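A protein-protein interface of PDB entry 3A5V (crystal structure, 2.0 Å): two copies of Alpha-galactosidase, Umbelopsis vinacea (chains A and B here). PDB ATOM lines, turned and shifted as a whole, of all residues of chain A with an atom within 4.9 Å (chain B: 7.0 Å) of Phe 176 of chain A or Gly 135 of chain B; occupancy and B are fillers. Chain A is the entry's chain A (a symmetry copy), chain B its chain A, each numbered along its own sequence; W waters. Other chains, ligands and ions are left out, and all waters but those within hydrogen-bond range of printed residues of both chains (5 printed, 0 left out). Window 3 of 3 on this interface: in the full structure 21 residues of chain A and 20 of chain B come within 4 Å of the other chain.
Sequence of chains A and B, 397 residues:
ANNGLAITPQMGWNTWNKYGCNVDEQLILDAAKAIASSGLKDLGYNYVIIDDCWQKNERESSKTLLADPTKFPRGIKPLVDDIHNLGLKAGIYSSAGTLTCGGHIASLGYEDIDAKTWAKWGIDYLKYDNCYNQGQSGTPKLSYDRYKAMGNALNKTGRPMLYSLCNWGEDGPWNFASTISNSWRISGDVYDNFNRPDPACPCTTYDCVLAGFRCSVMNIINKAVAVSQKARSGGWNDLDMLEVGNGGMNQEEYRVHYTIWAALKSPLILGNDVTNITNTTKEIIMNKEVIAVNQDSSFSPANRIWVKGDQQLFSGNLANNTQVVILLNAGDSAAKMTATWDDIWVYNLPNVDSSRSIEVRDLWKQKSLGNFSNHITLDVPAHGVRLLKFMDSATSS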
ATOM      1  N   PRO A 140      13.007 -12.661  18.255  1.00  0.00           N
ATOM      2  CA  PRO A 140      14.342 -12.790  17.662  1.00  0.00           C
ATOM      3  C   PRO A 140      14.385 -13.863  16.567  1.00  0.00           C
ATOM      4  O   PRO A 140      15.048 -13.666  15.542  1.00  0.00           O
ATOM      5  CB  PRO A 140      15.210 -13.208  18.859  1.00  0.00           C
ATOM      6  CG  PRO A 140      14.533 -12.548  20.022  1.00  0.00           C
ATOM      7  CD  PRO A 140      13.068 -12.722  19.730  1.00  0.00           C
ATOM      8  N   LYS A 141      13.679 -14.976  16.770  1.00  0.00           N
ATOM      9  CA  LYS A 141      13.662 -16.066  15.779  1.00  0.00           C
ATOM     10  C   LYS A 141      12.979 -15.688  14.461  1.00  0.00           C
ATOM     11  O   LYS A 141      13.493 -16.000  13.383  1.00  0.00           O
ATOM     12  CB  LYS A 141      13.029 -17.350  16.360  1.00  0.00           C
ATOM     13  CG  LYS A 141      13.097 -18.583  15.389  1.00  0.00           C
ATOM     14  CD  LYS A 141      14.531 -18.972  15.005  1.00  0.00           C
ATOM     15  CE  LYS A 141      14.583 -20.347  14.247  1.00  0.00           C
ATOM     16  NZ  LYS A 141      15.820 -20.448  13.373  1.00  0.00           N
ATOM     17  N   SER A 143      12.606 -12.608  13.167  1.00  0.00           N
ATOM     18  CA  SER A 143      13.444 -11.639  12.466  1.00  0.00           C
ATOM     19  C   SER A 143      14.735 -12.309  11.967  1.00  0.00           C
ATOM     20  O   SER A 143      15.163 -12.071  10.827  1.00  0.00           O
ATOM     21  CB  SER A 143      13.729 -10.412  13.347  1.00  0.00           C
ATOM     22  OG  SER A 143      12.544  -9.617  13.507  1.00  0.00           O
ATOM     23  N   TYR A 144      15.331 -13.163  12.805  1.00  0.00           N
ATOM     24  CA  TYR A 144      16.522 -13.924  12.399  1.00  0.00           C
ATOM     25  C   TYR A 144      16.326 -14.708  11.088  1.00  0.00           C
ATOM     26  O   TYR A 144      17.147 -14.612  10.183  1.00  0.00           O
ATOM     27  CB  TYR A 144      16.965 -14.887  13.509  1.00  0.00           C
ATOM     28  CG  TYR A 144      18.151 -15.745  13.128  1.00  0.00           C
ATOM     29  CD1 TYR A 144      17.966 -16.987  12.502  1.00  0.00           C
ATOM     30  CD2 TYR A 144      19.458 -15.327  13.404  1.00  0.00           C
ATOM     31  CE1 TYR A 144      19.058 -17.797  12.148  1.00  0.00           C
ATOM     32  CE2 TYR A 144      20.558 -16.120  13.047  1.00  0.00           C
ATOM     33  CZ  TYR A 144      20.337 -17.361  12.430  1.00  0.00           C
ATOM     34  OH  TYR A 144      21.402 -18.156  12.091  1.00  0.00           O
ATOM     35  N   TYR A 147      16.169 -12.413   7.957  1.00  0.00           N
ATOM     36  CA  TYR A 147      17.479 -11.823   7.623  1.00  0.00           C
ATOM     37  C   TYR A 147      18.528 -12.863   7.234  1.00  0.00           C
ATOM     38  O   TYR A 147      19.403 -12.584   6.418  1.00  0.00           O
ATOM     39  CB  TYR A 147      17.983 -10.853   8.725  1.00  0.00           C
ATOM     40  CG  TYR A 147      17.221  -9.553   8.641  1.00  0.00           C
ATOM     41  CD1 TYR A 147      17.443  -8.677   7.578  1.00  0.00           C
ATOM     42  CD2 TYR A 147      16.210  -9.240   9.556  1.00  0.00           C
ATOM     43  CE1 TYR A 147      16.709  -7.495   7.446  1.00  0.00           C
ATOM     44  CE2 TYR A 147      15.466  -8.050   9.428  1.00  0.00           C
ATOM     45  CZ  TYR A 147      15.720  -7.193   8.366  1.00  0.00           C
ATOM     46  OH  TYR A 147      14.998  -6.027   8.199  1.00  0.00           O
ATOM     47  N   LEU A 165      22.428  -4.657   8.048  1.00  0.00           N
ATOM     48  CA  LEU A 165      21.012  -4.760   8.449  1.00  0.00           C
ATOM     49  C   LEU A 165      20.424  -3.395   8.728  1.00  0.00           C
ATOM     50  O   LEU A 165      21.068  -2.539   9.350  1.00  0.00           O
ATOM     51  CB  LEU A 165      20.831  -5.652   9.688  1.00  0.00           C
ATOM     52  CG  LEU A 165      20.202  -7.016   9.422  1.00  0.00           C
ATOM     53  CD1 LEU A 165      21.047  -7.832   8.423  1.00  0.00           C
ATOM     54  CD2 LEU A 165      19.982  -7.773  10.710  1.00  0.00           C
ATOM     55  N   ASN A 167      17.001  -2.954  10.348  1.00  0.00           N
ATOM     56  CA  ASN A 167      15.743  -3.323  11.012  1.00  0.00           C
ATOM     57  C   ASN A 167      15.484  -2.518  12.302  1.00  0.00           C
ATOM     58  O   ASN A 167      14.606  -2.847  13.085  1.00  0.00           O
ATOM     59  CB  ASN A 167      15.648  -4.847  11.220  1.00  0.00           C
ATOM     60  CG  ASN A 167      16.086  -5.295  12.630  1.00  0.00           C
ATOM     61  OD1 ASN A 167      17.042  -4.764  13.212  1.00  0.00           O
ATOM     62  ND2 ASN A 167      15.378  -6.274  13.167  1.00  0.00           N
ATOM     63  N   GLU A 170      14.808  -3.820  15.977  1.00  0.00           N
ATOM     64  CA  GLU A 170      13.664  -4.679  16.303  1.00  0.00           C
ATOM     65  C   GLU A 170      14.114  -6.109  16.664  1.00  0.00           C
ATOM     66  O   GLU A 170      14.931  -6.702  15.968  1.00  0.00           O
ATOM     67  CB  GLU A 170      12.615  -4.691  15.179  1.00  0.00           C
ATOM     68  CG  GLU A 170      11.299  -5.405  15.566  1.00  0.00           C
ATOM     69  CD  GLU A 170      10.303  -5.524  14.404  1.00  0.00           C
ATOM     70  OE1 GLU A 170      10.714  -5.533  13.209  1.00  0.00           O
ATOM     71  OE2 GLU A 170       9.102  -5.649  14.701  1.00  0.00           O
ATOM     72  N   ASP A 171      13.601  -6.629  17.780  1.00  0.00           N
ATOM     73  CA  ASP A 171      13.930  -7.984  18.256  1.00  0.00           C
ATOM     74  C   ASP A 171      15.410  -8.221  18.617  1.00  0.00           C
ATOM     75  O   ASP A 171      15.834  -9.375  18.748  1.00  0.00           O
ATOM     76  CB  ASP A 171      13.461  -9.056  17.240  1.00  0.00           C
ATOM     77  CG  ASP A 171      11.969  -8.977  16.961  1.00  0.00           C
ATOM     78  OD1 ASP A 171      11.196  -8.882  17.935  1.00  0.00           O
ATOM     79  OD2 ASP A 171      11.567  -8.999  15.775  1.00  0.00           O
ATOM     80  N   GLY A 172      16.180  -7.142  18.766  1.00  0.00           N
ATOM     81  CA  GLY A 172      17.574  -7.223  19.245  1.00  0.00           C
ATOM     82  C   GLY A 172      18.587  -7.839  18.293  1.00  0.00           C
ATOM     83  O   GLY A 172      19.126  -8.922  18.579  1.00  0.00           O
ATOM     84  N   PRO A 173      18.885  -7.144  17.169  1.00  0.00           N
ATOM     85  CA  PRO A 173      19.871  -7.663  16.201  1.00  0.00           C
ATOM     86  C   PRO A 173      21.288  -7.791  16.790  1.00  0.00           C
ATOM     87  O   PRO A 173      22.049  -8.621  16.314  1.00  0.00           O
ATOM     88  CB  PRO A 173      19.849  -6.641  15.074  1.00  0.00           C
ATOM     89  CG  PRO A 173      19.339  -5.335  15.736  1.00  0.00           C
ATOM     90  CD  PRO A 173      18.344  -5.828  16.765  1.00  0.00           C
ATOM     91  N   TRP A 174      21.613  -7.003  17.822  1.00  0.00           N
ATOM     92  CA  TRP A 174      22.895  -7.136  18.549  1.00  0.00           C
ATOM     93  C   TRP A 174      23.075  -8.534  19.167  1.00  0.00           C
ATOM     94  O   TRP A 174      24.202  -8.942  19.464  1.00  0.00           O
ATOM     95  CB  TRP A 174      23.050  -6.031  19.626  1.00  0.00           C
ATOM     96  CG  TRP A 174      21.800  -5.842  20.442  1.00  0.00           C
ATOM     97  CD1 TRP A 174      21.402  -6.580  21.529  1.00  0.00           C
ATOM     98  CD2 TRP A 174      20.752  -4.897  20.189  1.00  0.00           C
ATOM     99  NE1 TRP A 174      20.178  -6.125  21.980  1.00  0.00           N
ATOM    100  CE2 TRP A 174      19.759  -5.096  21.175  1.00  0.00           C
ATOM    101  CE3 TRP A 174      20.571  -3.876  19.235  1.00  0.00           C
ATOM    102  CZ2 TRP A 174      18.592  -4.307  21.245  1.00  0.00           C
ATOM    103  CZ3 TRP A 174      19.414  -3.092  19.296  1.00  0.00           C
ATOM    104  CH2 TRP A 174      18.431  -3.318  20.294  1.00  0.00           C
ATOM    105  N   ASN A 175      21.961  -9.250  19.370  1.00  0.00           N
ATOM    106  CA  ASN A 175      21.973 -10.663  19.779  1.00  0.00           C
ATOM    107  C   ASN A 175      21.883 -11.610  18.570  1.00  0.00           C
ATOM    108  O   ASN A 175      22.709 -12.509  18.424  1.00  0.00           O
ATOM    109  CB  ASN A 175      20.817 -10.985  20.756  1.00  0.00           C
ATOM    110  CG  ASN A 175      20.809 -10.086  21.993  1.00  0.00           C
ATOM    111  OD1 ASN A 175      21.845  -9.863  22.644  1.00  0.00           O
ATOM    112  ND2 ASN A 175      19.622  -9.577  22.335  1.00  0.00           N
ATOM    113  N   PHE A 176      20.868 -11.423  17.718  1.00  0.00           N
ATOM    114  CA  PHE A 176      20.555 -12.428  16.697  1.00  0.00           C
ATOM    115  C   PHE A 176      21.355 -12.337  15.401  1.00  0.00           C
ATOM    116  O   PHE A 176      21.518 -13.340  14.697  1.00  0.00           O
ATOM    117  CB  PHE A 176      19.033 -12.563  16.425  1.00  0.00           C
ATOM    118  CG  PHE A 176      18.429 -11.443  15.566  1.00  0.00           C
ATOM    119  CD1 PHE A 176      18.689 -11.366  14.186  1.00  0.00           C
ATOM    120  CD2 PHE A 176      17.547 -10.507  16.138  1.00  0.00           C
ATOM    121  CE1 PHE A 176      18.107 -10.351  13.391  1.00  0.00           C
ATOM    122  CE2 PHE A 176      16.970  -9.461  15.346  1.00  0.00           C
ATOM    123  CZ  PHE A 176      17.263  -9.394  13.966  1.00  0.00           C
ATOM    124  N   ALA A 177      21.843 -11.141  15.086  1.00  0.00           N
ATOM    125  CA  ALA A 177      22.390 -10.869  13.742  1.00  0.00           C
ATOM    126  C   ALA A 177      23.918 -10.892  13.702  1.00  0.00           C
ATOM    127  O   ALA A 177      24.517 -10.721  12.648  1.00  0.00           O
ATOM    128  CB  ALA A 177      21.877  -9.514  13.231  1.00  0.00           C
ATOM    129  N   SER A 178      24.544 -11.118  14.852  1.00  0.00           N
ATOM    130  CA  SER A 178      25.974 -10.836  14.994  1.00  0.00           C
ATOM    131  C   SER A 178      26.884 -11.778  14.207  1.00  0.00           C
ATOM    132  O   SER A 178      27.998 -11.398  13.858  1.00  0.00           O
ATOM    133  CB  SER A 178      26.383 -10.813  16.470  1.00  0.00           C
ATOM    134  OG  SER A 178      25.927 -11.981  17.111  1.00  0.00           O
ATOM    135  N   ILE A 180      25.666 -13.406  11.381  1.00  0.00           N
ATOM    136  CA  ILE A 180      25.124 -13.525  10.013  1.00  0.00           C
ATOM    137  C   ILE A 180      25.148 -12.206   9.197  1.00  0.00           C
ATOM    138  O   ILE A 180      24.758 -12.198   8.036  1.00  0.00           O
ATOM    139  CB  ILE A 180      23.671 -14.107  10.028  1.00  0.00           C
ATOM    140  CG1 ILE A 180      22.736 -13.141  10.768  1.00  0.00           C
ATOM    141  CG2 ILE A 180      23.650 -15.571  10.617  1.00  0.00           C
ATOM    142  CD1 ILE A 180      21.241 -13.242  10.390  1.00  0.00           C
ATOM    143  N   TYR B 132      25.549 -15.983  21.081  1.00  0.00           N
ATOM    144  CA  TYR B 132      25.510 -16.376  19.667  1.00  0.00           C
ATOM    145  C   TYR B 132      24.486 -17.480  19.374  1.00  0.00           C
ATOM    146  O   TYR B 132      24.781 -18.451  18.676  1.00  0.00           O
ATOM    147  CB  TYR B 132      26.943 -16.705  19.156  1.00  0.00           C
ATOM    148  CG  TYR B 132      27.880 -15.523  19.356  1.00  0.00           C
ATOM    149  CD1 TYR B 132      27.662 -14.319  18.653  1.00  0.00           C
ATOM    150  CD2 TYR B 132      28.939 -15.570  20.275  1.00  0.00           C
ATOM    151  CE1 TYR B 132      28.485 -13.221  18.829  1.00  0.00           C
ATOM    152  CE2 TYR B 132      29.778 -14.448  20.468  1.00  0.00           C
ATOM    153  CZ  TYR B 132      29.534 -13.281  19.733  1.00  0.00           C
ATOM    154  OH  TYR B 132      30.330 -12.159  19.884  1.00  0.00           O
ATOM    155  N   ASN B 133      23.271 -17.294  19.899  1.00  0.00           N
ATOM    156  CA  ASN B 133      22.258 -18.347  19.890  1.00  0.00           C
ATOM    157  C   ASN B 133      21.370 -18.351  18.632  1.00  0.00           C
ATOM    158  O   ASN B 133      20.434 -19.136  18.526  1.00  0.00           O
ATOM    159  CB  ASN B 133      21.439 -18.346  21.211  1.00  0.00           C
ATOM    160  CG  ASN B 133      20.547 -17.121  21.371  1.00  0.00           C
ATOM    161  OD1 ASN B 133      19.990 -16.603  20.403  1.00  0.00           O
ATOM    162  ND2 ASN B 133      20.391 -16.664  22.616  1.00  0.00           N
ATOM    163  N   GLN B 134      21.694 -17.480  17.674  1.00  0.00           N
ATOM    164  CA  GLN B 134      21.076 -17.513  16.336  1.00  0.00           C
ATOM    165  C   GLN B 134      19.562 -17.240  16.420  1.00  0.00           C
ATOM    166  O   GLN B 134      18.739 -17.877  15.730  1.00  0.00           O
ATOM    167  CB  GLN B 134      21.405 -18.838  15.621  1.00  0.00           C
ATOM    168  CG  GLN B 134      22.918 -19.183  15.611  1.00  0.00           C
ATOM    169  CD  GLN B 134      23.758 -18.091  14.956  1.00  0.00           C
ATOM    170  OE1 GLN B 134      23.402 -17.590  13.883  1.00  0.00           O
ATOM    171  NE2 GLN B 134      24.877 -17.728  15.590  1.00  0.00           N
ATOM    172  N   GLY B 135      19.220 -16.266  17.264  1.00  0.00           N
ATOM    173  CA  GLY B 135      17.827 -15.857  17.480  1.00  0.00           C
ATOM    174  C   GLY B 135      16.931 -16.897  18.139  1.00  0.00           C
ATOM    175  O   GLY B 135      15.703 -16.748  18.119  1.00  0.00           O
ATOM    176  N   GLN B 136      17.516 -17.932  18.741  1.00  0.00           N
ATOM    177  CA  GLN B 136      16.709 -18.994  19.378  1.00  0.00           C
ATOM    178  C   GLN B 136      16.325 -18.670  20.834  1.00  0.00           C
ATOM    179  O   GLN B 136      16.635 -19.416  21.772  1.00  0.00           O
ATOM    180  CB  GLN B 136      17.383 -20.374  19.252  1.00  0.00           C
ATOM    181  CG  GLN B 136      17.468 -20.886  17.786  1.00  0.00           C
ATOM    182  CD  GLN B 136      18.200 -22.227  17.670  1.00  0.00           C
ATOM    183  OE1 GLN B 136      18.251 -23.001  18.624  1.00  0.00           O
ATOM    184  NE2 GLN B 136      18.765 -22.497  16.499  1.00  0.00           N
ATOM    185  N   SER B 137      15.634 -17.546  20.999  1.00  0.00           N
ATOM    186  CA  SER B 137      15.220 -17.036  22.305  1.00  0.00           C
ATOM    187  C   SER B 137      14.139 -15.991  22.046  1.00  0.00           C
ATOM    188  O   SER B 137      13.865 -15.670  20.885  1.00  0.00           O
ATOM    189  CB  SER B 137      16.422 -16.401  23.036  1.00  0.00           C
ATOM    190  OG  SER B 137      16.726 -15.111  22.511  1.00  0.00           O
ATOM    191  N   GLY B 138      13.516 -15.481  23.112  1.00  0.00           N
ATOM    192  CA  GLY B 138      12.463 -14.464  22.997  1.00  0.00           C
ATOM    193  C   GLY B 138      11.097 -14.972  23.451  1.00  0.00           C
ATOM    194  O   GLY B 138      10.184 -14.173  23.697  1.00  0.00           O
ATOM    195  N   LEU B 142      11.099 -21.158  22.881  1.00  0.00           N
ATOM    196  CA  LEU B 142      12.357 -21.106  22.100  1.00  0.00           C
ATOM    197  C   LEU B 142      13.596 -21.402  22.953  1.00  0.00           C
ATOM    198  O   LEU B 142      14.480 -22.199  22.553  1.00  0.00           O
ATOM    199  CB  LEU B 142      12.518 -19.754  21.372  1.00  0.00           C
ATOM    200  CG  LEU B 142      11.632 -19.503  20.139  1.00  0.00           C
ATOM    201  CD1 LEU B 142      11.576 -17.985  19.775  1.00  0.00           C
ATOM    202  CD2 LEU B 142      12.148 -20.313  18.963  1.00  0.00           C
ATOM    203  N   ARG B 146      16.121 -25.148  23.061  1.00  0.00           N
ATOM    204  CA  ARG B 146      17.574 -25.055  22.889  1.00  0.00           C
ATOM    205  C   ARG B 146      18.337 -25.636  24.093  1.00  0.00           C
ATOM    206  O   ARG B 146      19.332 -26.363  23.910  1.00  0.00           O
ATOM    207  CB  ARG B 146      17.977 -23.591  22.621  1.00  0.00           C
ATOM    208  CG  ARG B 146      19.495 -23.337  22.345  1.00  0.00           C
ATOM    209  CD  ARG B 146      19.727 -21.963  21.671  1.00  0.00           C
ATOM    210  NE  ARG B 146      18.957 -20.922  22.353  1.00  0.00           N
ATOM    211  CZ  ARG B 146      19.386 -20.231  23.403  1.00  0.00           C
ATOM    212  NH1 ARG B 146      20.624 -20.386  23.875  1.00  0.00           N
ATOM    213  NH2 ARG B 146      18.580 -19.344  23.966  1.00  0.00           N
HETATM  214  O   HOH W   1      22.668 -14.525  20.699  1.00  0.00           O
HETATM  215  O   HOH W   2      23.467 -15.096  17.342  1.00  0.00           O
HETATM  216  O   HOH W   3      18.312 -20.184  14.479  1.00  0.00           O
HETATM  217  O   HOH W   4      19.941 -14.146  19.492  1.00  0.00           O
HETATM  218  O   HOH W   5      23.936 -14.424  14.580  1.00  0.00           O
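OE1 of Gln 134 of chain B is in hydrogen-bond range of OH of Tyr 144 of chain A (2.7 Å).
N of Lys 141 of chain A is in hydrogen-bond range of O of Gly 135 of chain B.
O of Tyr 132 of chain B is in hydrogen-bond range of NE2 of Gln 134 of chain B (3.2 Å).
The side-chain amide oxygen (OD1) of Asn 133 of chain B lies within hydrogen-bond range of the backbone NH (N) of Gly 135 of chain B, 3.2 Å away.
Among the printed residues, pairs that only touch across the chains: Pro 140 of chain A with Ser 137 of chain B (3.3 Å), Ser 178 of chain A with Tyr 132 of chain B (3.3 Å), Pro 140 of chain A with Gly 135 of chain B (3.5 Å), Phe 176 of chain A with Gly 135 of chain B (3.7 Å), Pro 140 of chain A with Gly 138 of chain B (3.8 Å), Lys 141 of chain A with Leu 142 of chain B (3.8 Å), Ile 180 of chain A with Gln 134 of chain B (3.8 Å) and Tyr 144 of chain A with Gly 135 of chain B (3.98 Å).
Phe 176 of chain A touches just one residue of chain B: Gly 135 (3.7 Å).
Of chain A, only Pro 140, Lys 141, Tyr 144 and Phe 176 come within 4 Å of Gly 135 of chain B.
Of the printed residues of chain A, Leu 142 of chain B touches Lys 141.
Of the printed residues of chain A, Gly 138 of chain B touches Pro 140 (3.8 Å).
Printed residues of chain B within 4 Å of Tyr 144 of chain A: Gln 134 and Gly 135.
Of the printed residues of chain B, Ile 180 of chain A touches Gln 134 (3.8 Å).
Printed residues of chain A within 4 Å of Tyr 132 of chain B: Ser 178.
Tyr 147 of chain A touches none of the printed residues of chain B.
The nearest residue of chain B that does not touch Phe 176 of chain A is Gln 134 of chain B (4.5 Å).
The nearest printed residue of chain A that does not touch Gly 138 of chain B is Lys 141 of chain A (6.4 Å).
Of the 9 printed residues of chain B, 6 touch a printed residue of chain A.
Hydrophobic or aromatic side chains of chain B within 4 Å of the printed part of chain A: Tyr 132 and Leu 142.
Among the printed residues, 10 pairs touch across the chains.
Among the printed residues, no Asp or Glu carboxylate lies within 4 Å of a Lys or Arg side-chain nitrogen of the other chain.
No position is printed for both chains.
Of the 10 pairs that touch across the chains among the printed residues, none has its exchanged pair printed and touching as well.
Water W4 lies within hydrogen-bond range of OD1 of Asn 133 of chain B, N of Gly 135 of chain B, N of Phe 176 of chain A and O of Asn 175 of chain A.
Water W5 lies within hydrogen-bond range of O of Phe 176 of chain A (2.7 Å), OE1 of Gln 134 of chain B (3.3 Å) and N of Ser 178 of chain A (3.4 Å).
Water W3 lies within hydrogen-bond range of the backbone carbonyl oxygen of Gln 134 of chain B (2.7 Å), the side-chain amino group of Lys 141 of chain A (2.7 Å) and the side-chain amide nitrogen of Gln 136 of chain B (3.1 Å).
Water W2 lies within hydrogen-bond range of O of Asn 175 of chain A (2.9 Å), N of Gln 134 of chain B (3.0 Å) and N of Asn 133 of chain B (3.4 Å).
Water W1 lies within hydrogen-bond range of N of Asn 133 of chain B (2.9 Å), O of Asn 175 of chain A (3.0 Å) and N of Tyr 132 of chain B (3.3 Å).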
